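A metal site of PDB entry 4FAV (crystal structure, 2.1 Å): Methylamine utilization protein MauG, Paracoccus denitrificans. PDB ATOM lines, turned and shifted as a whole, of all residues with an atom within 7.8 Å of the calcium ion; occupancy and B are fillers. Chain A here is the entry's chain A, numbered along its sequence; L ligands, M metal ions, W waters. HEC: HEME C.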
ATOM      1  N   ARG A  39      25.081  -8.653  -6.475  1.00  0.00           N
ATOM      2  CA  ARG A  39      24.025  -7.641  -6.588  1.00  0.00           C
ATOM      3  C   ARG A  39      23.673  -7.327  -8.045  1.00  0.00           C
ATOM      4  O   ARG A  39      23.428  -6.169  -8.405  1.00  0.00           O
ATOM      5  CB  ARG A  39      24.435  -6.345  -5.891  1.00  0.00           C
ATOM      6  CG  ARG A  39      23.234  -5.579  -5.350  1.00  0.00           C
ATOM      7  CD  ARG A  39      23.644  -4.260  -4.774  1.00  0.00           C
ATOM      8  NE  ARG A  39      22.520  -3.489  -4.239  1.00  0.00           N
ATOM      9  CZ  ARG A  39      21.820  -2.577  -4.916  1.00  0.00           C
ATOM     10  NH1 ARG A  39      22.115  -2.301  -6.169  1.00  0.00           N
ATOM     11  NH2 ARG A  39      20.809  -1.908  -4.319  1.00  0.00           N
ATOM     12  N   THR A  42      25.762  -4.595  -9.661  1.00  0.00           N
ATOM     13  CA  THR A  42      25.662  -3.196  -9.271  1.00  0.00           C
ATOM     14  C   THR A  42      26.324  -3.069  -7.919  1.00  0.00           C
ATOM     15  O   THR A  42      26.710  -4.079  -7.315  1.00  0.00           O
ATOM     16  CB  THR A  42      24.220  -2.697  -9.159  1.00  0.00           C
ATOM     17  OG1 THR A  42      23.510  -3.496  -8.196  1.00  0.00           O
ATOM     18  CG2 THR A  42      23.541  -2.746 -10.483  1.00  0.00           C
ATOM     19  N   ASP A  43      26.378  -1.825  -7.433  1.00  0.00           N
ATOM     20  CA  ASP A  43      27.156  -1.470  -6.266  1.00  0.00           C
ATOM     21  C   ASP A  43      26.309  -1.500  -5.020  1.00  0.00           C
ATOM     22  O   ASP A  43      25.346  -0.688  -4.884  1.00  0.00           O
ATOM     23  CB  ASP A  43      27.826  -0.113  -6.459  1.00  0.00           C
ATOM     24  CG  ASP A  43      28.928   0.170  -5.380  1.00  0.00           C
ATOM     25  OD1 ASP A  43      29.658   1.181  -5.536  1.00  0.00           O
ATOM     26  OD2 ASP A  43      29.034  -0.609  -4.399  1.00  0.00           O
ATOM     27  N   LEU A  51      23.135   4.790  -2.156  1.00  0.00           N
ATOM     28  CA  LEU A  51      23.582   3.897  -3.223  1.00  0.00           C
ATOM     29  C   LEU A  51      23.308   4.509  -4.555  1.00  0.00           C
ATOM     30  O   LEU A  51      23.370   3.824  -5.585  1.00  0.00           O
ATOM     31  CB  LEU A  51      22.899   2.534  -3.094  1.00  0.00           C
ATOM     32  CG  LEU A  51      22.962   1.959  -1.668  1.00  0.00           C
ATOM     33  CD1 LEU A  51      22.269   0.601  -1.600  1.00  0.00           C
ATOM     34  CD2 LEU A  51      24.402   1.821  -1.162  1.00  0.00           C
ATOM     35  N   ALA A  52      23.024   5.820  -4.521  1.00  0.00           N
ATOM     36  CA  ALA A  52      22.716   6.609  -5.680  1.00  0.00           C
ATOM     37  C   ALA A  52      23.942   6.594  -6.574  1.00  0.00           C
ATOM     38  O   ALA A  52      23.795   6.344  -7.780  1.00  0.00           O
ATOM     39  CB  ALA A  52      22.330   8.033  -5.327  1.00  0.00           C
ATOM     40  N   ASN A  66      24.350   6.686 -11.293  1.00  0.00           N
ATOM     41  CA  ASN A  66      24.159   5.418 -10.605  1.00  0.00           C
ATOM     42  C   ASN A  66      24.729   4.298 -11.447  1.00  0.00           C
ATOM     43  O   ASN A  66      24.640   4.346 -12.718  1.00  0.00           O
ATOM     44  CB  ASN A  66      22.677   5.182 -10.349  1.00  0.00           C
ATOM     45  CG  ASN A  66      22.403   3.824  -9.787  1.00  0.00           C
ATOM     46  OD1 ASN A  66      21.781   2.978 -10.454  1.00  0.00           O
ATOM     47  ND2 ASN A  66      22.940   3.560  -8.568  1.00  0.00           N
ATOM     48  N   THR A  67      25.338   3.323 -10.747  1.00  0.00           N
ATOM     49  CA  THR A  67      26.061   2.198 -11.343  1.00  0.00           C
ATOM     50  C   THR A  67      25.027   1.235 -11.931  1.00  0.00           C
ATOM     51  O   THR A  67      24.189   0.705 -11.211  1.00  0.00           O
ATOM     52  CB  THR A  67      26.984   1.546 -10.292  1.00  0.00           C
ATOM     53  OG1 THR A  67      28.043   2.458  -9.928  1.00  0.00           O
ATOM     54  CG2 THR A  67      27.583   0.160 -10.759  1.00  0.00           C
ATOM     55  N   PRO A  68      24.979   1.118 -13.290  1.00  0.00           N
ATOM     56  CA  PRO A  68      24.037   0.187 -13.849  1.00  0.00           C
ATOM     57  C   PRO A  68      24.504  -1.275 -13.795  1.00  0.00           C
ATOM     58  O   PRO A  68      25.694  -1.593 -13.695  1.00  0.00           O
ATOM     59  CB  PRO A  68      23.903   0.677 -15.336  1.00  0.00           C
ATOM     60  CG  PRO A  68      25.295   1.189 -15.623  1.00  0.00           C
ATOM     61  CD  PRO A  68      25.904   1.649 -14.284  1.00  0.00           C
ATOM     62  N   THR A  69      23.542  -2.189 -13.862  1.00  0.00           N
ATOM     63  CA  THR A  69      23.849  -3.611 -14.017  1.00  0.00           C
ATOM     64  C   THR A  69      24.618  -3.903 -15.325  1.00  0.00           C
ATOM     65  O   THR A  69      24.485  -3.186 -16.296  1.00  0.00           O
ATOM     66  CB  THR A  69      22.608  -4.392 -14.110  1.00  0.00           C
ATOM     67  OG1 THR A  69      22.993  -5.749 -14.158  1.00  0.00           O
ATOM     68  CG2 THR A  69      21.827  -3.976 -15.505  1.00  0.00           C
ATOM     69  N   TRP A  93      24.919   5.514 -19.486  1.00  0.00           N
ATOM     70  CA  TRP A  93      23.604   6.073 -19.515  1.00  0.00           C
ATOM     71  C   TRP A  93      23.458   7.146 -20.599  1.00  0.00           C
ATOM     72  O   TRP A  93      22.336   7.473 -21.002  1.00  0.00           O
ATOM     73  CB  TRP A  93      23.377   6.724 -18.188  1.00  0.00           C
ATOM     74  CG  TRP A  93      23.076   5.837 -17.034  1.00  0.00           C
ATOM     75  CD1 TRP A  93      23.932   5.492 -15.997  1.00  0.00           C
ATOM     76  CD2 TRP A  93      21.821   5.277 -16.733  1.00  0.00           C
ATOM     77  NE1 TRP A  93      23.264   4.714 -15.077  1.00  0.00           N
ATOM     78  CE2 TRP A  93      21.965   4.580 -15.493  1.00  0.00           C
ATOM     79  CE3 TRP A  93      20.564   5.308 -17.359  1.00  0.00           C
ATOM     80  CZ2 TRP A  93      20.882   3.895 -14.889  1.00  0.00           C
ATOM     81  CZ3 TRP A  93      19.485   4.616 -16.743  1.00  0.00           C
ATOM     82  CH2 TRP A  93      19.656   3.959 -15.516  1.00  0.00           C
ATOM     83  N   VAL A 272      15.563  -5.410 -12.730  1.00  0.00           N
ATOM     84  CA  VAL A 272      15.243  -4.052 -12.242  1.00  0.00           C
ATOM     85  C   VAL A 272      14.817  -4.096 -10.799  1.00  0.00           C
ATOM     86  O   VAL A 272      15.051  -3.118 -10.043  1.00  0.00           O
ATOM     87  CB  VAL A 272      14.194  -3.317 -13.080  1.00  0.00           C
ATOM     88  CG1 VAL A 272      12.817  -4.033 -13.050  1.00  0.00           C
ATOM     89  CG2 VAL A 272      14.086  -1.808 -12.640  1.00  0.00           C
ATOM     90  N   VAL A 274      16.153  -5.687  -8.484  1.00  0.00           N
ATOM     91  CA  VAL A 274      17.208  -5.812  -7.488  1.00  0.00           C
ATOM     92  C   VAL A 274      18.319  -4.770  -7.675  1.00  0.00           C
ATOM     93  O   VAL A 274      19.295  -4.780  -6.926  1.00  0.00           O
ATOM     94  CB  VAL A 274      17.785  -7.280  -7.414  1.00  0.00           C
ATOM     95  CG1 VAL A 274      16.665  -8.333  -7.279  1.00  0.00           C
ATOM     96  CG2 VAL A 274      18.673  -7.558  -8.581  1.00  0.00           C
ATOM     97  N   THR A 275      18.171  -3.848  -8.628  1.00  0.00           N
ATOM     98  CA  THR A 275      19.257  -2.906  -8.856  1.00  0.00           C
ATOM     99  C   THR A 275      18.897  -1.449  -8.495  1.00  0.00           C
ATOM    100  O   THR A 275      19.387  -0.495  -9.122  1.00  0.00           O
ATOM    101  CB  THR A 275      19.653  -2.955 -10.263  1.00  0.00           C
ATOM    102  OG1 THR A 275      18.475  -2.739 -11.009  1.00  0.00           O
ATOM    103  CG2 THR A 275      20.178  -4.292 -10.600  1.00  0.00           C
ATOM    104  N   GLY A 276      18.047  -1.270  -7.497  1.00  0.00           N
ATOM    105  CA  GLY A 276      17.767   0.065  -6.959  1.00  0.00           C
ATOM    106  C   GLY A 276      19.051   0.637  -6.417  1.00  0.00           C
ATOM    107  O   GLY A 276      20.001  -0.113  -6.163  1.00  0.00           O
ATOM    108  N   PRO A 277      19.106   1.971  -6.231  1.00  0.00           N
ATOM    109  CA  PRO A 277      18.078   2.902  -6.583  1.00  0.00           C
ATOM    110  C   PRO A 277      18.017   3.118  -8.116  1.00  0.00           C
ATOM    111  O   PRO A 277      18.804   2.526  -8.891  1.00  0.00           O
ATOM    112  CB  PRO A 277      18.473   4.156  -5.788  1.00  0.00           C
ATOM    113  CG  PRO A 277      19.847   4.068  -5.589  1.00  0.00           C
ATOM    114  CD  PRO A 277      20.233   2.644  -5.580  1.00  0.00           C
ATOM    115  N   TYR A 278      17.046   3.904  -8.566  1.00  0.00           N
ATOM    116  CA  TYR A 278      16.720   3.920  -9.985  1.00  0.00           C
ATOM    117  C   TYR A 278      16.995   5.233 -10.701  1.00  0.00           C
ATOM    118  O   TYR A 278      17.253   6.272 -10.070  1.00  0.00           O
ATOM    119  CB  TYR A 278      15.287   3.461 -10.185  1.00  0.00           C
ATOM    120  CG  TYR A 278      15.077   2.103  -9.602  1.00  0.00           C
ATOM    121  CD1 TYR A 278      14.626   1.967  -8.312  1.00  0.00           C
ATOM    122  CD2 TYR A 278      15.430   0.951 -10.309  1.00  0.00           C
ATOM    123  CE1 TYR A 278      14.468   0.733  -7.749  1.00  0.00           C
ATOM    124  CE2 TYR A 278      15.249  -0.291  -9.759  1.00  0.00           C
ATOM    125  CZ  TYR A 278      14.791  -0.385  -8.454  1.00  0.00           C
ATOM    126  OH  TYR A 278      14.612  -1.619  -7.868  1.00  0.00           O
ATOM    127  N   MET A 279      16.937   5.135 -12.040  1.00  0.00           N
ATOM    128  CA  MET A 279      17.204   6.227 -12.947  1.00  0.00           C
ATOM    129  C   MET A 279      18.695   6.504 -13.021  1.00  0.00           C
ATOM    130  O   MET A 279      19.495   6.010 -12.197  1.00  0.00           O
ATOM    131  CB  MET A 279      16.394   7.470 -12.544  1.00  0.00           C
ATOM    132  CG  MET A 279      14.848   7.218 -12.629  1.00  0.00           C
ATOM    133  SD  MET A 279      14.302   6.390 -14.148  1.00  0.00           S
ATOM    134  CE  MET A 279      12.577   6.038 -13.809  1.00  0.00           C
ATOM    135  N   HIS A 280      19.072   7.320 -13.978  1.00  0.00           N
ATOM    136  CA  HIS A 280      20.476   7.580 -14.247  1.00  0.00           C
ATOM    137  C   HIS A 280      21.188   8.114 -13.002  1.00  0.00           C
ATOM    138  O   HIS A 280      22.405   8.053 -12.888  1.00  0.00           O
ATOM    139  CB  HIS A 280      20.629   8.533 -15.452  1.00  0.00           C
ATOM    140  CG  HIS A 280      20.144   9.930 -15.164  1.00  0.00           C
ATOM    141  ND1 HIS A 280      18.891  10.390 -15.541  1.00  0.00           N
ATOM    142  CD2 HIS A 280      20.750  10.966 -14.528  1.00  0.00           C
ATOM    143  CE1 HIS A 280      18.741  11.636 -15.147  1.00  0.00           C
ATOM    144  NE2 HIS A 280      19.850  12.019 -14.522  1.00  0.00           N
ATOM    145  N   ASN A 281      20.442   8.638 -12.060  1.00  0.00           N
ATOM    146  CA  ASN A 281      21.081   9.296 -10.942  1.00  0.00           C
ATOM    147  C   ASN A 281      20.675   8.688  -9.600  1.00  0.00           C
ATOM    148  O   ASN A 281      20.870   9.308  -8.576  1.00  0.00           O
ATOM    149  CB  ASN A 281      20.806  10.805 -10.960  1.00  0.00           C
ATOM    150  CG  ASN A 281      19.316  11.121 -10.949  1.00  0.00           C
ATOM    151  OD1 ASN A 281      18.489  10.233 -10.684  1.00  0.00           O
ATOM    152  ND2 ASN A 281      18.972  12.380 -11.228  1.00  0.00           N
ATOM    153  N   GLY A 282      20.101   7.500  -9.623  1.00  0.00           N
ATOM    154  CA  GLY A 282      19.718   6.855  -8.389  1.00  0.00           C
ATOM    155  C   GLY A 282      18.716   7.625  -7.555  1.00  0.00           C
ATOM    156  O   GLY A 282      18.562   7.317  -6.395  1.00  0.00           O
ATOM    157  N   PHE A 284      15.460   7.597  -7.212  1.00  0.00           N
ATOM    158  CA  PHE A 284      14.372   6.850  -6.531  1.00  0.00           C
ATOM    159  C   PHE A 284      14.892   5.543  -5.947  1.00  0.00           C
ATOM    160  O   PHE A 284      15.496   4.720  -6.673  1.00  0.00           O
ATOM    161  CB  PHE A 284      13.175   6.563  -7.467  1.00  0.00           C
ATOM    162  CG  PHE A 284      12.731   7.755  -8.249  1.00  0.00           C
ATOM    163  CD1 PHE A 284      12.476   8.972  -7.606  1.00  0.00           C
ATOM    164  CD2 PHE A 284      12.533   7.674  -9.608  1.00  0.00           C
ATOM    165  CE1 PHE A 284      12.045  10.070  -8.307  1.00  0.00           C
ATOM    166  CE2 PHE A 284      12.108   8.782 -10.339  1.00  0.00           C
ATOM    167  CZ  PHE A 284      11.873   9.999  -9.686  1.00  0.00           C
HETATM  168 FE   HEC L   1      10.790   3.740 -18.252  1.00  0.00          FE
HETATM  169  CHA HEC L   1      13.768   4.130 -16.573  1.00  0.00           C
HETATM  170  CHB HEC L   1       9.672   1.573 -15.957  1.00  0.00           C
HETATM  171  CHC HEC L   1       7.558   4.078 -19.566  1.00  0.00           C
HETATM  172  CHD HEC L   1      12.037   5.283 -20.966  1.00  0.00           C
HETATM  173  NA  HEC L   1      11.579   2.989 -16.493  1.00  0.00           N
HETATM  174  C1A HEC L   1      12.781   3.201 -15.999  1.00  0.00           C
HETATM  175  C2A HEC L   1      13.037   2.454 -14.746  1.00  0.00           C
HETATM  176  C3A HEC L   1      11.881   1.719 -14.539  1.00  0.00           C
HETATM  177  C4A HEC L   1      11.008   2.118 -15.700  1.00  0.00           C
HETATM  178  CMA HEC L   1      11.583   0.751 -13.444  1.00  0.00           C
HETATM  179  CAA HEC L   1      14.308   2.488 -13.976  1.00  0.00           C
HETATM  180  CBA HEC L   1      15.181   1.365 -14.553  1.00  0.00           C
HETATM  181  CGA HEC L   1      16.550   1.457 -13.917  1.00  0.00           C
HETATM  182  O1A HEC L   1      16.753   2.432 -13.178  1.00  0.00           O
HETATM  183  O2A HEC L   1      17.447   0.575 -14.133  1.00  0.00           O
HETATM  184  NB  HEC L   1       8.951   2.972 -17.839  1.00  0.00           N
HETATM  185  C1B HEC L   1       8.681   2.074 -16.899  1.00  0.00           C
HETATM  186  C2B HEC L   1       7.306   1.628 -16.864  1.00  0.00           C
HETATM  187  C3B HEC L   1       6.699   2.363 -17.865  1.00  0.00           C
HETATM  188  C4B HEC L   1       7.785   3.185 -18.409  1.00  0.00           C
HETATM  189  CMB HEC L   1       6.723   0.618 -15.931  1.00  0.00           C
HETATM  190  CAB HEC L   1       5.273   2.356 -18.333  1.00  0.00           C
HETATM  191  CBB HEC L   1       4.480   2.969 -17.184  1.00  0.00           C
HETATM  192  NC  HEC L   1       9.976   4.512 -20.008  1.00  0.00           N
HETATM  193  C1C HEC L   1       8.669   4.601 -20.342  1.00  0.00           C
HETATM  194  C2C HEC L   1       8.423   5.292 -21.578  1.00  0.00           C
HETATM  195  C3C HEC L   1       9.672   5.639 -22.034  1.00  0.00           C
HETATM  196  C4C HEC L   1      10.587   5.149 -20.981  1.00  0.00           C
HETATM  197  CMC HEC L   1       7.054   5.485 -22.153  1.00  0.00           C
HETATM  198  CAC HEC L   1       9.983   6.378 -23.322  1.00  0.00           C
HETATM  199  CBC HEC L   1       9.165   7.633 -23.363  1.00  0.00           C
HETATM  200  ND  HEC L   1      12.638   4.526 -18.691  1.00  0.00           N
HETATM  201  C1D HEC L   1      12.924   5.249 -19.790  1.00  0.00           C
HETATM  202  C2D HEC L   1      14.250   5.873 -19.761  1.00  0.00           C
HETATM  203  C3D HEC L   1      14.723   5.541 -18.506  1.00  0.00           C
HETATM  204  C4D HEC L   1      13.679   4.712 -17.897  1.00  0.00           C
HETATM  205  CMD HEC L   1      14.925   6.720 -20.813  1.00  0.00           C
HETATM  206  CAD HEC L   1      16.013   6.003 -17.890  1.00  0.00           C
HETATM  207  CBD HEC L   1      15.593   7.438 -17.529  1.00  0.00           C
HETATM  208  CGD HEC L   1      16.751   8.152 -16.900  1.00  0.00           C
HETATM  209  O1D HEC L   1      17.397   7.559 -16.012  1.00  0.00           O
HETATM  210  O2D HEC L   1      17.044   9.300 -17.286  1.00  0.00           O
HETATM  211 CA    CA M   1      20.236   1.285 -10.261  1.00  0.00          CA
HETATM  212  O   HOH W   1      21.632   0.841  -8.267  1.00  0.00           O
HETATM  213  O   HOH W   2      19.380   2.696 -11.913  1.00  0.00           O
HETATM  214  O   HOH W   3      21.766  -0.168 -11.234  1.00  0.00           O
HETATM  215  O   HOH W   4      18.809  -0.045 -11.395  1.00  0.00           O
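The backbone NH of Met 279 is in hydrogen-bond range of an oxygen (O1A) of the ligand, 2.9 Å away.
N of His 280 sits at hydrogen-bond distance from O1D of the ligand, 2.6 Å away.
A ring nitrogen (ND1) of His 280 lies within hydrogen-bond range of an oxygen (O2D) of the ligand.
NE1 of Trp 93 is in hydrogen-bond range of O of Asn 66 (2.8 Å).
The backbone carbonyl oxygen of Leu 51 is in hydrogen-bond range of the side-chain amide nitrogen of Asn 66 (3.0 Å).
ND2 of Asn 66 lies close to O of Ala 52 (3.0 Å).
N of Asn 66 lies within hydrogen-bond range of O of His 280 (2.9 Å).
Three residues have an atom within 4 Å of the calcium ion: Asn 66, Thr 275 and Pro 277.
The nearest printed residue that does not touch the calcium ion is Gly 276 (4.1 Å).
The calcium ion is bound by water W4, the backbone carbonyl oxygen of Thr 275, the side-chain amide oxygen of Asn 66, water W3, water W2, the backbone carbonyl oxygen of Pro 277 and water W1.
The calcium ion has seven donor atoms within binding distance.
Water W4 bridges the side-chain hydroxyl of Thr 275 (2.7 Å) and an oxygen (O2A) of the ligand (3.1 Å).
Water W1 lies within hydrogen-bond range of O of Gly 276 (2.8 Å) and ND2 of Asn 66 (3.0 Å).
Water W2 bridges an oxygen (O1A) of the ligand and the backbone carbonyl oxygen (O) of Met 279.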
